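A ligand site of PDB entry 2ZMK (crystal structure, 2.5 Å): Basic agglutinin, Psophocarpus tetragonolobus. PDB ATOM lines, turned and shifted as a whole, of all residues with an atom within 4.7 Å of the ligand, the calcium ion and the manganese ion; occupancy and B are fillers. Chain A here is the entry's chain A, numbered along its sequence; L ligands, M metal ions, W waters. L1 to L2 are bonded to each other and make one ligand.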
ATOM      1  N   HIS A  84      24.907   1.196 -15.715  1.00  0.00           N
ATOM      2  CA  HIS A  84      24.280   0.811 -16.974  1.00  0.00           C
ATOM      3  C   HIS A  84      25.181   0.929 -18.204  1.00  0.00           C
ATOM      4  O   HIS A  84      25.784   1.976 -18.473  1.00  0.00           O
ATOM      5  CB  HIS A  84      23.027   1.662 -17.180  1.00  0.00           C
ATOM      6  CG  HIS A  84      23.263   3.131 -17.021  1.00  0.00           C
ATOM      7  ND1 HIS A  84      22.415   3.949 -16.308  1.00  0.00           N
ATOM      8  CD2 HIS A  84      24.250   3.940 -17.478  1.00  0.00           C
ATOM      9  CE1 HIS A  84      22.867   5.189 -16.339  1.00  0.00           C
ATOM     10  NE2 HIS A  84      23.984   5.214 -17.045  1.00  0.00           N
ATOM     11  N   ALA A  86      26.248   1.330 -22.171  1.00  0.00           N
ATOM     12  CA  ALA A  86      25.706   2.188 -23.224  1.00  0.00           C
ATOM     13  C   ALA A  86      26.728   2.329 -24.356  1.00  0.00           C
ATOM     14  O   ALA A  86      27.921   2.153 -24.128  1.00  0.00           O
ATOM     15  CB  ALA A  86      25.368   3.567 -22.640  1.00  0.00           C
ATOM     16  N   ASP A  87      26.277   2.633 -25.574  1.00  0.00           N
ATOM     17  CA  ASP A  87      24.873   2.825 -25.917  1.00  0.00           C
ATOM     18  C   ASP A  87      24.373   1.761 -26.899  1.00  0.00           C
ATOM     19  O   ASP A  87      23.173   1.459 -26.946  1.00  0.00           O
ATOM     20  CB  ASP A  87      24.666   4.204 -26.524  1.00  0.00           C
ATOM     21  CG  ASP A  87      24.329   5.251 -25.482  1.00  0.00           C
ATOM     22  OD1 ASP A  87      25.267   5.832 -24.899  1.00  0.00           O
ATOM     23  OD2 ASP A  87      23.131   5.479 -25.227  1.00  0.00           O
ATOM     24  N   GLY A 104      26.163   9.069 -27.902  1.00  0.00           N
ATOM     25  CA  GLY A 104      25.156   8.622 -26.972  1.00  0.00           C
ATOM     26  C   GLY A 104      24.057   7.784 -27.609  1.00  0.00           C
ATOM     27  O   GLY A 104      24.321   6.928 -28.468  1.00  0.00           O
ATOM     28  N   GLY A 105      22.821   8.023 -27.201  1.00  0.00           N
ATOM     29  CA  GLY A 105      21.693   7.285 -27.721  1.00  0.00           C
ATOM     30  C   GLY A 105      21.418   7.500 -29.192  1.00  0.00           C
ATOM     31  O   GLY A 105      20.518   6.871 -29.754  1.00  0.00           O
ATOM     32  N   PHE A 107      23.799   7.031 -31.428  1.00  0.00           N
ATOM     33  CA  PHE A 107      24.761   6.131 -32.076  1.00  0.00           C
ATOM     34  C   PHE A 107      25.743   6.774 -33.050  1.00  0.00           C
ATOM     35  O   PHE A 107      26.539   6.069 -33.658  1.00  0.00           O
ATOM     36  CB  PHE A 107      24.001   5.029 -32.809  1.00  0.00           C
ATOM     37  CG  PHE A 107      22.930   4.364 -31.995  1.00  0.00           C
ATOM     38  CD1 PHE A 107      23.266   3.570 -30.898  1.00  0.00           C
ATOM     39  CD2 PHE A 107      21.586   4.503 -32.347  1.00  0.00           C
ATOM     40  CE1 PHE A 107      22.267   2.916 -30.157  1.00  0.00           C
ATOM     41  CE2 PHE A 107      20.595   3.862 -31.616  1.00  0.00           C
ATOM     42  CZ  PHE A 107      20.931   3.068 -30.519  1.00  0.00           C
ATOM     43  N   GLU A 122      19.501  -1.254 -35.353  1.00  0.00           N
ATOM     44  CA  GLU A 122      20.234  -1.012 -34.126  1.00  0.00           C
ATOM     45  C   GLU A 122      20.186  -2.151 -33.134  1.00  0.00           C
ATOM     46  O   GLU A 122      19.242  -2.945 -33.102  1.00  0.00           O
ATOM     47  CB  GLU A 122      19.672   0.231 -33.421  1.00  0.00           C
ATOM     48  CG  GLU A 122      18.228   0.043 -33.018  1.00  0.00           C
ATOM     49  CD  GLU A 122      17.689   1.172 -32.165  1.00  0.00           C
ATOM     50  OE1 GLU A 122      17.731   2.338 -32.605  1.00  0.00           O
ATOM     51  OE2 GLU A 122      17.225   0.870 -31.052  1.00  0.00           O
ATOM     52  N   ASP A 124      20.472  -1.869 -29.515  1.00  0.00           N
ATOM     53  CA  ASP A 124      20.397  -0.916 -28.433  1.00  0.00           C
ATOM     54  C   ASP A 124      20.595  -1.505 -27.057  1.00  0.00           C
ATOM     55  O   ASP A 124      19.882  -2.429 -26.664  1.00  0.00           O
ATOM     56  CB  ASP A 124      19.054  -0.215 -28.487  1.00  0.00           C
ATOM     57  CG  ASP A 124      19.124   1.169 -27.935  1.00  0.00           C
ATOM     58  OD1 ASP A 124      19.918   1.387 -26.999  1.00  0.00           O
ATOM     59  OD2 ASP A 124      18.395   2.036 -28.452  1.00  0.00           O
ATOM     60  N   PHE A 126      21.175   0.734 -24.103  1.00  0.00           N
ATOM     61  CA  PHE A 126      20.828   1.679 -23.060  1.00  0.00           C
ATOM     62  C   PHE A 126      19.411   2.171 -23.267  1.00  0.00           C
ATOM     63  O   PHE A 126      19.032   2.520 -24.378  1.00  0.00           O
ATOM     64  CB  PHE A 126      21.767   2.885 -23.103  1.00  0.00           C
ATOM     65  CG  PHE A 126      21.446   3.915 -22.080  1.00  0.00           C
ATOM     66  CD1 PHE A 126      21.746   3.685 -20.738  1.00  0.00           C
ATOM     67  CD2 PHE A 126      20.814   5.100 -22.435  1.00  0.00           C
ATOM     68  CE1 PHE A 126      21.420   4.624 -19.766  1.00  0.00           C
ATOM     69  CE2 PHE A 126      20.486   6.051 -21.471  1.00  0.00           C
ATOM     70  CZ  PHE A 126      20.786   5.811 -20.130  1.00  0.00           C
ATOM     71  N   ARG A 127      18.618   2.225 -22.200  1.00  0.00           N
ATOM     72  CA  ARG A 127      17.246   2.673 -22.357  1.00  0.00           C
ATOM     73  C   ARG A 127      17.032   4.175 -22.239  1.00  0.00           C
ATOM     74  O   ARG A 127      17.018   4.731 -21.137  1.00  0.00           O
ATOM     75  CB  ARG A 127      16.334   1.950 -21.357  1.00  0.00           C
ATOM     76  CG  ARG A 127      14.878   2.298 -21.554  1.00  0.00           C
ATOM     77  CD  ARG A 127      13.959   1.437 -20.724  1.00  0.00           C
ATOM     78  NE  ARG A 127      12.556   1.690 -21.064  1.00  0.00           N
ATOM     79  CZ  ARG A 127      11.534   1.013 -20.545  1.00  0.00           C
ATOM     80  NH1 ARG A 127      11.755   0.047 -19.667  1.00  0.00           N
ATOM     81  NH2 ARG A 127      10.289   1.304 -20.913  1.00  0.00           N
ATOM     82  N   ASN A 128      16.851   4.836 -23.379  1.00  0.00           N
ATOM     83  CA  ASN A 128      16.589   6.266 -23.392  1.00  0.00           C
ATOM     84  C   ASN A 128      15.091   6.446 -23.167  1.00  0.00           C
ATOM     85  O   ASN A 128      14.355   5.463 -23.068  1.00  0.00           O
ATOM     86  CB  ASN A 128      16.995   6.886 -24.736  1.00  0.00           C
ATOM     87  CG  ASN A 128      18.497   7.015 -24.870  1.00  0.00           C
ATOM     88  OD1 ASN A 128      19.203   6.021 -25.006  1.00  0.00           O
ATOM     89  ND2 ASN A 128      19.000   8.251 -24.800  1.00  0.00           N
ATOM     90  N   THR A 129      14.644   7.696 -23.103  1.00  0.00           N
ATOM     91  CA  THR A 129      13.231   7.972 -22.870  1.00  0.00           C
ATOM     92  C   THR A 129      12.322   7.404 -23.960  1.00  0.00           C
ATOM     93  O   THR A 129      11.187   6.978 -23.681  1.00  0.00           O
ATOM     94  CB  THR A 129      12.968   9.492 -22.777  1.00  0.00           C
ATOM     95  OG1 THR A 129      13.347  10.139 -23.999  1.00  0.00           O
ATOM     96  CG2 THR A 129      13.770  10.094 -21.627  1.00  0.00           C
ATOM     97  N   TRP A 130      12.829   7.368 -25.184  1.00  0.00           N
ATOM     98  CA  TRP A 130      12.059   6.876 -26.329  1.00  0.00           C
ATOM     99  C   TRP A 130      12.187   5.362 -26.563  1.00  0.00           C
ATOM    100  O   TRP A 130      11.654   4.831 -27.541  1.00  0.00           O
ATOM    101  CB  TRP A 130      12.521   7.618 -27.586  1.00  0.00           C
ATOM    102  CG  TRP A 130      13.981   7.421 -27.868  1.00  0.00           C
ATOM    103  CD1 TRP A 130      14.575   6.293 -28.353  1.00  0.00           C
ATOM    104  CD2 TRP A 130      15.028   8.355 -27.621  1.00  0.00           C
ATOM    105  NE1 TRP A 130      15.936   6.470 -28.435  1.00  0.00           N
ATOM    106  CE2 TRP A 130      16.246   7.730 -27.993  1.00  0.00           C
ATOM    107  CE3 TRP A 130      15.079   9.671 -27.133  1.00  0.00           C
ATOM    108  CZ2 TRP A 130      17.480   8.366 -27.891  1.00  0.00           C
ATOM    109  CZ3 TRP A 130      16.314  10.307 -27.031  1.00  0.00           C
ATOM    110  CH2 TRP A 130      17.499   9.656 -27.410  1.00  0.00           C
ATOM    111  N   ASP A 131      12.884   4.680 -25.653  1.00  0.00           N
ATOM    112  CA  ASP A 131      13.116   3.251 -25.781  1.00  0.00           C
ATOM    113  C   ASP A 131      12.309   2.316 -24.925  1.00  0.00           C
ATOM    114  O   ASP A 131      11.852   2.686 -23.842  1.00  0.00           O
ATOM    115  CB  ASP A 131      14.572   2.882 -25.439  1.00  0.00           C
ATOM    116  CG  ASP A 131      15.550   3.257 -26.505  1.00  0.00           C
ATOM    117  OD1 ASP A 131      15.231   3.090 -27.708  1.00  0.00           O
ATOM    118  OD2 ASP A 131      16.647   3.690 -26.131  1.00  0.00           O
ATOM    119  N   HIS A 136      17.652  -4.406 -27.132  1.00  0.00           N
ATOM    120  CA  HIS A 136      16.650  -4.699 -28.142  1.00  0.00           C
ATOM    121  C   HIS A 136      17.166  -4.411 -29.540  1.00  0.00           C
ATOM    122  O   HIS A 136      18.078  -3.595 -29.718  1.00  0.00           O
ATOM    123  CB  HIS A 136      15.363  -3.911 -27.894  1.00  0.00           C
ATOM    124  CG  HIS A 136      15.524  -2.420 -27.921  1.00  0.00           C
ATOM    125  ND1 HIS A 136      15.436  -1.653 -26.781  1.00  0.00           N
ATOM    126  CD2 HIS A 136      15.750  -1.571 -28.946  1.00  0.00           C
ATOM    127  CE1 HIS A 136      15.592  -0.374 -27.111  1.00  0.00           C
ATOM    128  NE2 HIS A 136      15.782  -0.302 -28.420  1.00  0.00           N
ATOM    129  N   VAL A 144      15.927   7.595 -34.428  1.00  0.00           N
ATOM    130  CA  VAL A 144      16.330   6.600 -33.461  1.00  0.00           C
ATOM    131  C   VAL A 144      15.104   6.027 -32.752  1.00  0.00           C
ATOM    132  O   VAL A 144      15.218   5.104 -31.950  1.00  0.00           O
ATOM    133  CB  VAL A 144      17.329   7.243 -32.456  1.00  0.00           C
ATOM    134  CG1 VAL A 144      17.465   6.401 -31.226  1.00  0.00           C
ATOM    135  CG2 VAL A 144      18.692   7.372 -33.136  1.00  0.00           C
ATOM    136  N   SER A 146      12.668   3.711 -33.109  1.00  0.00           N
ATOM    137  CA  SER A 146      12.377   2.554 -33.949  1.00  0.00           C
ATOM    138  C   SER A 146      10.926   2.363 -34.355  1.00  0.00           C
ATOM    139  O   SER A 146      10.019   2.674 -33.602  1.00  0.00           O
ATOM    140  CB  SER A 146      12.863   1.281 -33.240  1.00  0.00           C
ATOM    141  OG  SER A 146      14.191   1.437 -32.827  1.00  0.00           O
ATOM    142  N   THR A 210      29.423   5.105 -26.915  1.00  0.00           N
ATOM    143  CA  THR A 210      29.427   4.737 -25.518  1.00  0.00           C
ATOM    144  C   THR A 210      28.794   5.877 -24.740  1.00  0.00           C
ATOM    145  O   THR A 210      28.471   6.920 -25.325  1.00  0.00           O
ATOM    146  CB  THR A 210      30.860   4.477 -25.006  1.00  0.00           C
ATOM    147  OG1 THR A 210      31.710   5.578 -25.356  1.00  0.00           O
ATOM    148  CG2 THR A 210      31.405   3.206 -25.626  1.00  0.00           C
ATOM    149  N   GLY A 211      28.612   5.684 -23.440  1.00  0.00           N
ATOM    150  CA  GLY A 211      27.987   6.688 -22.601  1.00  0.00           C
ATOM    151  C   GLY A 211      28.389   8.128 -22.838  1.00  0.00           C
ATOM    152  O   GLY A 211      29.554   8.438 -23.014  1.00  0.00           O
ATOM    153  N   ASP A 212      27.388   9.007 -22.856  1.00  0.00           N
ATOM    154  CA  ASP A 212      27.626  10.427 -23.050  1.00  0.00           C
ATOM    155  C   ASP A 212      28.017  11.051 -21.700  1.00  0.00           C
ATOM    156  O   ASP A 212      27.459  10.698 -20.656  1.00  0.00           O
ATOM    157  CB  ASP A 212      26.362  11.102 -23.581  1.00  0.00           C
ATOM    158  CG  ASP A 212      26.632  12.494 -24.090  1.00  0.00           C
ATOM    159  OD1 ASP A 212      27.243  12.617 -25.169  1.00  0.00           O
ATOM    160  OD2 ASP A 212      26.247  13.464 -23.392  1.00  0.00           O
ATOM    161  N   SER A 214      27.316  13.791 -20.335  1.00  0.00           N
ATOM    162  CA  SER A 214      26.180  14.433 -19.684  1.00  0.00           C
ATOM    163  C   SER A 214      25.538  13.548 -18.620  1.00  0.00           C
ATOM    164  O   SER A 214      24.912  14.030 -17.686  1.00  0.00           O
ATOM    165  CB  SER A 214      25.127  14.843 -20.711  1.00  0.00           C
ATOM    166  OG  SER A 214      24.523  13.712 -21.303  1.00  0.00           O
ATOM    167  N   GLY A 215      25.686  12.233 -18.782  1.00  0.00           N
ATOM    168  CA  GLY A 215      25.107  11.304 -17.821  1.00  0.00           C
ATOM    169  C   GLY A 215      26.012  11.142 -16.619  1.00  0.00           C
ATOM    170  O   GLY A 215      25.638  10.514 -15.629  1.00  0.00           O
ATOM    171  N   GLN A 217      28.521   9.304 -15.951  1.00  0.00           N
ATOM    172  CA  GLN A 217      28.723   7.912 -15.571  1.00  0.00           C
ATOM    173  C   GLN A 217      29.793   7.251 -16.452  1.00  0.00           C
ATOM    174  O   GLN A 217      29.492   6.747 -17.524  1.00  0.00           O
ATOM    175  CB  GLN A 217      27.416   7.124 -15.708  1.00  0.00           C
ATOM    176  CG  GLN A 217      26.459   7.324 -14.560  1.00  0.00           C
ATOM    177  CD  GLN A 217      27.076   6.928 -13.241  1.00  0.00           C
ATOM    178  OE1 GLN A 217      27.914   6.017 -13.173  1.00  0.00           O
ATOM    179  NE2 GLN A 217      26.657   7.584 -12.168  1.00  0.00           N
ATOM    180  N   ALA A 220      29.213   3.865 -18.004  1.00  0.00           N
ATOM    181  CA  ALA A 220      28.257   3.711 -19.102  1.00  0.00           C
ATOM    182  C   ALA A 220      29.029   3.478 -20.385  1.00  0.00           C
ATOM    183  O   ALA A 220      29.119   4.350 -21.237  1.00  0.00           O
ATOM    184  CB  ALA A 220      27.400   4.953 -19.229  1.00  0.00           C
HETATM  185  C1  LIG L   1      19.857   9.737 -18.845  1.00  0.00           C
HETATM  186  C2  LIG L   1      21.332  10.091 -18.536  1.00  0.00           C
HETATM  187  C3  LIG L   1      21.874  10.983 -19.654  1.00  0.00           C
HETATM  188  O1  LIG L   1      19.642  11.842 -20.072  1.00  0.00           O
HETATM  189  C4  LIG L   1      16.753  11.724 -19.624  1.00  0.00           C
HETATM  190  C5  LIG L   1      15.574  11.537 -18.669  1.00  0.00           C
HETATM  191  C6  LIG L   1      19.056  11.029 -19.029  1.00  0.00           C
HETATM  192  C7  LIG L   1      21.002  12.232 -19.764  1.00  0.00           C
HETATM  193  C8  LIG L   1      21.491  13.202 -20.849  1.00  0.00           C
HETATM  194  O2  LIG L   1      17.742  10.733 -19.362  1.00  0.00           O
HETATM  195  O3  LIG L   1      19.306   8.972 -17.790  1.00  0.00           O
HETATM  196  O4  LIG L   1      22.120   8.918 -18.427  1.00  0.00           O
HETATM  197  O5  LIG L   1      21.835  10.257 -20.907  1.00  0.00           O
HETATM  198  O6  LIG L   1      20.426  13.671 -21.667  1.00  0.00           O
HETATM  199  C1  LG2 L   2      23.001  10.290 -21.659  1.00  0.00           C
HETATM  200  C2  LG2 L   2      22.709   9.801 -23.093  1.00  0.00           C
HETATM  201  C3  LG2 L   2      22.361   8.300 -23.066  1.00  0.00           C
HETATM  202  C4  LG2 L   2      23.498   7.532 -22.402  1.00  0.00           C
HETATM  203  C5  LG2 L   2      23.721   8.080 -20.987  1.00  0.00           C
HETATM  204  C6  LG2 L   2      24.864   7.402 -20.262  1.00  0.00           C
HETATM  205  O1  LG2 L   2      21.625  10.543 -23.651  1.00  0.00           O
HETATM  206  O2  LG2 L   2      22.163   7.825 -24.397  1.00  0.00           O
HETATM  207  O3  LG2 L   2      24.693   7.676 -23.157  1.00  0.00           O
HETATM  208  O4  LG2 L   2      24.033   9.492 -21.066  1.00  0.00           O
HETATM  209  O5  LG2 L   2      24.971   7.871 -18.927  1.00  0.00           O
HETATM  210 CA    CA M   1      19.144   3.779 -26.535  1.00  0.00          CA
HETATM  211 MN    MN M   2      16.214   1.729 -29.183  1.00  0.00          MN
HETATM  212  O   HOH W   1      16.850   3.565 -30.284  1.00  0.00           O
HETATM  213  O   HOH W   2      18.683   5.127 -28.866  1.00  0.00           O
HETATM  214  O   HOH W   3      21.870   4.178 -26.967  1.00  0.00           O
HETATM  215  O   HOH W   4      14.286   2.016 -30.461  1.00  0.00           O
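C of Gly 104 touches O2 of LG2 L2, at 3.7 Å.
Thr 129 touches the ligand.
CA of Gly 211 touches O3 of LG2 L2, 3.5 Å away.
OG of Ser 214 touches C8 of LIG L1 (3.1 Å).
Gly 215 touches the ligand.
CB of Ala 220 touches C6 of LG2 L2, 3.7 Å away.
Within 4 Å of the ligand: His 84, Asp 87, Gly 104, Gly 105, Phe 126, Asn 128, Thr 129, Gly 211, Asp 212, Ser 214, Gly 215 and Ala 220.
The nearest printed residue that does not touch the ligand is Gln 217 (4.1 Å).
The nearest printed residue that does not touch the calcium ion is Phe 107 (4.4 Å).
The calcium ion is bound by the backbone carbonyl oxygen (O) of Phe 126 (2.5 Å), the side-chain carboxylate (OD2) of Asp 131 (2.5 Å), the side-chain carboxylate (OD1) of Asp 124 (2.6 Å), the side-chain carboxylate (OD2) of Asp 124 (2.7 Å), the side-chain amide oxygen (OD1) of Asn 128 (2.7 Å), water W2 (2.7 Å) and water W3 (2.8 Å).
The calcium ion has seven donor atoms within binding distance.
The nearest printed residue that does not touch the manganese ion is Ser 146 (4.2 Å).
A ring nitrogen (NE2) of His 84 lies within hydrogen-bond range of an oxygen (O5) of LG2 L2.
The backbone NH of Gly 105 sits at hydrogen-bond distance from an oxygen (O2) of LG2 L2 (2.9 Å).
The backbone NH (N) of Asp 212 sits at hydrogen-bond distance from an oxygen (O3) of LG2 L2 (3.0 Å).
O2 of LG2 L2 lies within hydrogen-bond range of ND2 of Asn 128, at 3.2 Å.
An oxygen (O3) of LG2 L2 is in hydrogen-bond range of the side-chain carboxylate (OD1) of Asp 87 (2.6 Å).
The manganese ion is bound by NE2 of His 136, water W1, OD1 of Asp 131, OE2 of Glu 122, OD2 of Asp 124 and water W4.
The manganese ion has six donor atoms within binding distance.
The side-chain hydroxyl (OG) of Ser 214 is in hydrogen-bond range of the side-chain carboxylate (OD2) of Asp 212, at 2.7 Å.
N of Gly 211 sits at hydrogen-bond distance from O of Ala 220 (2.6 Å).
O of Asp 131 is in hydrogen-bond range of NE of Arg 127 (3.0 Å).
OD2 of Asp 87 sits at hydrogen-bond distance from N of Gly 105 (3.2 Å).
Water W2 bridges O of Gly 105 (2.7 Å) and NE1 of Trp 130 (3.1 Å).
Water W1 lies within hydrogen-bond range of the side-chain carboxylate of Glu 122 (2.8 Å) and the backbone carbonyl oxygen of Val 144 (2.8 Å).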
